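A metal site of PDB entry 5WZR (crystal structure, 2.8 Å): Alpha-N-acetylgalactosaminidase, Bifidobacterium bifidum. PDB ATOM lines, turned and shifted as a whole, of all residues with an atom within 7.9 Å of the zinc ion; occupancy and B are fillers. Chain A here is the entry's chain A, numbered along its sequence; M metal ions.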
ATOM      1  N   ARG A 382      11.577 -11.987  19.013  1.00  0.00           N
ATOM      2  CA  ARG A 382      11.581 -11.807  20.474  1.00  0.00           C
ATOM      3  C   ARG A 382      12.919 -11.247  21.004  1.00  0.00           C
ATOM      4  O   ARG A 382      12.974 -10.780  22.142  1.00  0.00           O
ATOM      5  CB  ARG A 382      11.213 -13.122  21.221  1.00  0.00           C
ATOM      6  CG  ARG A 382      12.409 -14.019  21.538  1.00  0.00           C
ATOM      7  CD  ARG A 382      12.071 -15.304  22.289  1.00  0.00           C
ATOM      8  NE  ARG A 382      11.094 -15.089  23.361  1.00  0.00           N
ATOM      9  CZ  ARG A 382       9.975 -15.807  23.558  1.00  0.00           C
ATOM     10  NH1 ARG A 382       9.673 -16.844  22.766  1.00  0.00           N
ATOM     11  NH2 ARG A 382       9.162 -15.507  24.569  1.00  0.00           N
ATOM     12  N   ASN A 383      13.988 -11.314  20.197  1.00  0.00           N
ATOM     13  CA  ASN A 383      15.268 -10.619  20.514  1.00  0.00           C
ATOM     14  C   ASN A 383      15.400  -9.176  19.990  1.00  0.00           C
ATOM     15  O   ASN A 383      16.420  -8.492  20.209  1.00  0.00           O
ATOM     16  CB  ASN A 383      16.452 -11.427  19.995  1.00  0.00           C
ATOM     17  CG  ASN A 383      16.514 -12.807  20.592  1.00  0.00           C
ATOM     18  OD1 ASN A 383      15.888 -13.071  21.616  1.00  0.00           O
ATOM     19  ND2 ASN A 383      17.271 -13.703  19.954  1.00  0.00           N
ATOM     20  N   ALA A 384      14.383  -8.693  19.297  1.00  0.00           N
ATOM     21  CA  ALA A 384      14.519  -7.446  18.602  1.00  0.00           C
ATOM     22  C   ALA A 384      13.970  -6.281  19.400  1.00  0.00           C
ATOM     23  O   ALA A 384      13.079  -6.443  20.246  1.00  0.00           O
ATOM     24  CB  ALA A 384      13.836  -7.533  17.267  1.00  0.00           C
ATOM     25  N   ILE A 385      14.545  -5.117  19.145  1.00  0.00           N
ATOM     26  CA  ILE A 385      14.019  -3.868  19.614  1.00  0.00           C
ATOM     27  C   ILE A 385      12.521  -3.791  19.322  1.00  0.00           C
ATOM     28  O   ILE A 385      12.066  -4.166  18.237  1.00  0.00           O
ATOM     29  CB  ILE A 385      14.690  -2.652  18.910  1.00  0.00           C
ATOM     30  CG1 ILE A 385      16.114  -2.414  19.437  1.00  0.00           C
ATOM     31  CG2 ILE A 385      13.870  -1.382  19.074  1.00  0.00           C
ATOM     32  CD1 ILE A 385      16.207  -2.099  20.923  1.00  0.00           C
ATOM     33  N   ARG A 386      11.788  -3.309  20.310  1.00  0.00           N
ATOM     34  CA  ARG A 386      10.505  -2.672  20.071  1.00  0.00           C
ATOM     35  C   ARG A 386      10.637  -1.228  20.408  1.00  0.00           C
ATOM     36  O   ARG A 386      11.260  -0.882  21.420  1.00  0.00           O
ATOM     37  CB  ARG A 386       9.430  -3.285  20.938  1.00  0.00           C
ATOM     38  CG  ARG A 386       9.188  -4.733  20.616  1.00  0.00           C
ATOM     39  CD  ARG A 386       8.899  -4.961  19.144  1.00  0.00           C
ATOM     40  NE  ARG A 386       8.523  -6.360  18.973  1.00  0.00           N
ATOM     41  CZ  ARG A 386       9.375  -7.383  18.959  1.00  0.00           C
ATOM     42  NH1 ARG A 386      10.688  -7.150  19.067  1.00  0.00           N
ATOM     43  NH2 ARG A 386       8.928  -8.619  18.835  1.00  0.00           N
ATOM     44  N   TYR A 405      16.740  -4.404  14.511  1.00  0.00           N
ATOM     45  CA  TYR A 405      17.875  -4.043  15.366  1.00  0.00           C
ATOM     46  C   TYR A 405      17.887  -4.861  16.624  1.00  0.00           C
ATOM     47  O   TYR A 405      16.904  -4.907  17.344  1.00  0.00           O
ATOM     48  CB  TYR A 405      17.823  -2.597  15.802  1.00  0.00           C
ATOM     49  CG  TYR A 405      17.797  -1.591  14.697  1.00  0.00           C
ATOM     50  CD1 TYR A 405      18.624  -1.708  13.605  1.00  0.00           C
ATOM     51  CD2 TYR A 405      16.939  -0.507  14.761  1.00  0.00           C
ATOM     52  CE1 TYR A 405      18.583  -0.783  12.574  1.00  0.00           C
ATOM     53  CE2 TYR A 405      16.885   0.424  13.740  1.00  0.00           C
ATOM     54  CZ  TYR A 405      17.700   0.289  12.651  1.00  0.00           C
ATOM     55  OH  TYR A 405      17.642   1.232  11.649  1.00  0.00           O
ATOM     56  N   LEU A 406      19.014  -5.475  16.917  1.00  0.00           N
ATOM     57  CA  LEU A 406      19.130  -6.342  18.057  1.00  0.00           C
ATOM     58  C   LEU A 406      19.092  -5.526  19.346  1.00  0.00           C
ATOM     59  O   LEU A 406      19.826  -4.552  19.490  1.00  0.00           O
ATOM     60  CB  LEU A 406      20.455  -7.093  17.969  1.00  0.00           C
ATOM     61  CG  LEU A 406      20.750  -8.054  19.116  1.00  0.00           C
ATOM     62  CD1 LEU A 406      19.719  -9.146  19.187  1.00  0.00           C
ATOM     63  CD2 LEU A 406      22.107  -8.666  18.892  1.00  0.00           C
ATOM     64  N   CYS A 407      18.249  -5.913  20.298  1.00  0.00           N
ATOM     65  CA  CYS A 407      18.245  -5.183  21.569  1.00  0.00           C
ATOM     66  C   CYS A 407      19.643  -5.275  22.171  1.00  0.00           C
ATOM     67  O   CYS A 407      20.192  -6.355  22.323  1.00  0.00           O
ATOM     68  CB  CYS A 407      17.180  -5.706  22.542  1.00  0.00           C
ATOM     69  SG  CYS A 407      16.862  -4.551  23.910  1.00  0.00           S
ATOM     70  N   ALA A 408      20.244  -4.146  22.478  1.00  0.00           N
ATOM     71  CA  ALA A 408      21.584  -4.129  23.015  1.00  0.00           C
ATOM     72  C   ALA A 408      21.691  -4.896  24.332  1.00  0.00           C
ATOM     73  O   ALA A 408      22.731  -5.453  24.640  1.00  0.00           O
ATOM     74  CB  ALA A 408      22.054  -2.707  23.209  1.00  0.00           C
ATOM     75  N   GLU A 409      20.625  -4.949  25.097  1.00  0.00           N
ATOM     76  CA  GLU A 409      20.657  -5.747  26.331  1.00  0.00           C
ATOM     77  C   GLU A 409      21.218  -7.132  26.075  1.00  0.00           C
ATOM     78  O   GLU A 409      21.777  -7.780  26.967  1.00  0.00           O
ATOM     79  CB  GLU A 409      19.254  -5.881  26.901  1.00  0.00           C
ATOM     80  CG  GLU A 409      18.730  -4.597  27.526  1.00  0.00           C
ATOM     81  CD  GLU A 409      19.334  -4.322  28.875  1.00  0.00           C
ATOM     82  OE1 GLU A 409      19.395  -5.255  29.683  1.00  0.00           O
ATOM     83  OE2 GLU A 409      19.762  -3.180  29.147  1.00  0.00           O
ATOM     84  N   LEU A 410      21.024  -7.597  24.851  1.00  0.00           N
ATOM     85  CA  LEU A 410      21.424  -8.929  24.472  1.00  0.00           C
ATOM     86  C   LEU A 410      22.706  -8.969  23.651  1.00  0.00           C
ATOM     87  O   LEU A 410      23.266 -10.064  23.480  1.00  0.00           O
ATOM     88  CB  LEU A 410      20.313  -9.570  23.671  1.00  0.00           C
ATOM     89  CG  LEU A 410      18.922  -9.634  24.280  1.00  0.00           C
ATOM     90  CD1 LEU A 410      17.990 -10.452  23.390  1.00  0.00           C
ATOM     91  CD2 LEU A 410      18.992 -10.216  25.660  1.00  0.00           C
ATOM     92  N   GLU A 444      16.195   2.599  22.138  1.00  0.00           N
ATOM     93  CA  GLU A 444      15.421   2.357  23.347  1.00  0.00           C
ATOM     94  C   GLU A 444      14.502   1.217  23.025  1.00  0.00           C
ATOM     95  O   GLU A 444      14.151   1.035  21.894  1.00  0.00           O
ATOM     96  CB  GLU A 444      14.672   3.619  23.834  1.00  0.00           C
ATOM     97  CG  GLU A 444      13.442   4.049  23.047  1.00  0.00           C
ATOM     98  CD  GLU A 444      12.806   5.324  23.578  1.00  0.00           C
ATOM     99  OE1 GLU A 444      13.300   5.916  24.555  1.00  0.00           O
ATOM    100  OE2 GLU A 444      11.789   5.754  23.005  1.00  0.00           O
ATOM    101  N   CYS A 445      14.131   0.447  24.029  1.00  0.00           N
ATOM    102  CA  CYS A 445      13.429  -0.805  23.837  1.00  0.00           C
ATOM    103  C   CYS A 445      12.332  -0.969  24.855  1.00  0.00           C
ATOM    104  O   CYS A 445      12.608  -0.843  26.059  1.00  0.00           O
ATOM    105  CB  CYS A 445      14.409  -1.975  23.994  1.00  0.00           C
ATOM    106  SG  CYS A 445      13.742  -3.554  23.479  1.00  0.00           S
ATOM    107  N   SER A 446      11.120  -1.263  24.388  1.00  0.00           N
ATOM    108  CA  SER A 446       9.984  -1.408  25.273  1.00  0.00           C
ATOM    109  C   SER A 446       9.561  -2.846  25.444  1.00  0.00           C
ATOM    110  O   SER A 446       8.577  -3.132  26.112  1.00  0.00           O
ATOM    111  CB  SER A 446       8.816  -0.599  24.716  1.00  0.00           C
ATOM    112  OG  SER A 446       8.480  -1.049  23.435  1.00  0.00           O
ATOM    113  N   HIS A 447      10.293  -3.775  24.833  1.00  0.00           N
ATOM    114  CA  HIS A 447      10.022  -5.194  25.015  1.00  0.00           C
ATOM    115  C   HIS A 447      10.249  -5.556  26.503  1.00  0.00           C
ATOM    116  O   HIS A 447      11.289  -5.220  27.062  1.00  0.00           O
ATOM    117  CB  HIS A 447      10.933  -6.037  24.118  1.00  0.00           C
ATOM    118  CG  HIS A 447      10.426  -7.408  23.856  1.00  0.00           C
ATOM    119  ND1 HIS A 447      10.169  -8.323  24.858  1.00  0.00           N
ATOM    120  CD2 HIS A 447      10.117  -8.046  22.695  1.00  0.00           C
ATOM    121  CE1 HIS A 447       9.709  -9.446  24.340  1.00  0.00           C
ATOM    122  NE2 HIS A 447       9.676  -9.308  23.032  1.00  0.00           N
ATOM    123  N   PRO A 448       9.295  -6.235  27.142  1.00  0.00           N
ATOM    124  CA  PRO A 448       9.415  -6.430  28.599  1.00  0.00           C
ATOM    125  C   PRO A 448      10.529  -7.406  29.013  1.00  0.00           C
ATOM    126  O   PRO A 448      11.172  -7.228  30.081  1.00  0.00           O
ATOM    127  CB  PRO A 448       8.049  -7.007  28.996  1.00  0.00           C
ATOM    128  CG  PRO A 448       7.196  -6.966  27.780  1.00  0.00           C
ATOM    129  CD  PRO A 448       8.086  -6.887  26.592  1.00  0.00           C
ATOM    130  N   GLU A 449      10.721  -8.431  28.187  1.00  0.00           N
ATOM    131  CA  GLU A 449      11.852  -9.324  28.293  1.00  0.00           C
ATOM    132  C   GLU A 449      13.234  -8.661  28.205  1.00  0.00           C
ATOM    133  O   GLU A 449      14.184  -9.225  28.752  1.00  0.00           O
ATOM    134  CB  GLU A 449      11.735 -10.407  27.237  1.00  0.00           C
ATOM    135  CG  GLU A 449      10.618 -11.382  27.495  1.00  0.00           C
ATOM    136  CD  GLU A 449      10.441 -12.390  26.389  1.00  0.00           C
ATOM    137  OE1 GLU A 449      11.187 -12.299  25.378  1.00  0.00           O
ATOM    138  OE2 GLU A 449       9.550 -13.265  26.520  1.00  0.00           O
ATOM    139  N   HIS A 450      13.367  -7.503  27.545  1.00  0.00           N
ATOM    140  CA  HIS A 450      14.648  -6.756  27.560  1.00  0.00           C
ATOM    141  C   HIS A 450      14.483  -5.218  27.368  1.00  0.00           C
ATOM    142  O   HIS A 450      15.067  -4.603  26.451  1.00  0.00           O
ATOM    143  CB  HIS A 450      15.594  -7.343  26.529  1.00  0.00           C
ATOM    144  CG  HIS A 450      14.883  -7.792  25.294  1.00  0.00           C
ATOM    145  ND1 HIS A 450      14.322  -6.914  24.395  1.00  0.00           N
ATOM    146  CD2 HIS A 450      14.602  -9.036  24.840  1.00  0.00           C
ATOM    147  CE1 HIS A 450      13.738  -7.590  23.426  1.00  0.00           C
ATOM    148  NE2 HIS A 450      13.885  -8.877  23.669  1.00  0.00           N
ATOM    149  N   ARG A 451      13.700  -4.625  28.269  1.00  0.00           N
ATOM    150  CA  ARG A 451      13.393  -3.200  28.264  1.00  0.00           C
ATOM    151  C   ARG A 451      14.678  -2.409  28.414  1.00  0.00           C
ATOM    152  O   ARG A 451      15.526  -2.786  29.229  1.00  0.00           O
ATOM    153  CB  ARG A 451      12.419  -2.869  29.409  1.00  0.00           C
ATOM    154  CG  ARG A 451      12.077  -1.387  29.548  1.00  0.00           C
ATOM    155  CD  ARG A 451      10.974  -1.019  30.571  1.00  0.00           C
ATOM    156  NE  ARG A 451      11.341  -1.063  32.012  1.00  0.00           N
ATOM    157  CZ  ARG A 451      12.423  -0.526  32.598  1.00  0.00           C
ATOM    158  NH1 ARG A 451      13.385   0.102  31.895  1.00  0.00           N
ATOM    159  NH2 ARG A 451      12.563  -0.649  33.909  1.00  0.00           N
ATOM    160  N   MET A 452      14.859  -1.343  27.644  1.00  0.00           N
ATOM    161  CA  MET A 452      16.159  -0.631  27.664  1.00  0.00           C
ATOM    162  C   MET A 452      16.097   0.802  27.200  1.00  0.00           C
ATOM    163  O   MET A 452      15.687   1.063  26.081  1.00  0.00           O
ATOM    164  CB  MET A 452      17.182  -1.338  26.791  1.00  0.00           C
ATOM    165  CG  MET A 452      18.481  -0.578  26.570  1.00  0.00           C
ATOM    166  SD  MET A 452      19.550  -1.385  25.366  1.00  0.00           S
ATOM    167  CE  MET A 452      18.756  -0.946  23.839  1.00  0.00           C
ATOM    168  N   THR A 453      16.593   1.712  28.045  1.00  0.00           N
ATOM    169  CA  THR A 453      16.630   3.132  27.751  1.00  0.00           C
ATOM    170  C   THR A 453      17.818   3.411  26.863  1.00  0.00           C
ATOM    171  O   THR A 453      18.728   2.598  26.773  1.00  0.00           O
ATOM    172  CB  THR A 453      16.705   4.014  29.045  1.00  0.00           C
ATOM    173  OG1 THR A 453      17.950   3.847  29.737  1.00  0.00           O
ATOM    174  CG2 THR A 453      15.559   3.672  29.982  1.00  0.00           C
HETATM  175 ZN    ZN M   1      14.994  -4.953  24.463  1.00  0.00          ZN
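N of Arg 386 sits close to SG of Cys 445 (3.7 Å).
The backbone carbonyl oxygen of Met 452 lies within hydrogen-bond range of the backbone NH of Cys 445 (2.6 Å).
The backbone NH of Cys 407 lies within hydrogen-bond range of the backbone carbonyl oxygen of Asn 383 (3.2 Å).
The backbone NH of His 447 sits close to the side-chain sulfur of Cys 445 (3.7 Å).
A ring nitrogen (NE2) of His 450 lies within hydrogen-bond range of the backbone carbonyl oxygen of Arg 382, 2.6 Å away.
Three residues have an atom within 4 Å of the zinc ion: Cys 407, Cys 445 and His 450.
The nearest printed residue that does not touch the zinc ion is Arg 451 (4.03 Å).
The zinc ion is bound by SG of Cys 407, O of His 450, ND1 of His 450 and SG of Cys 445.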
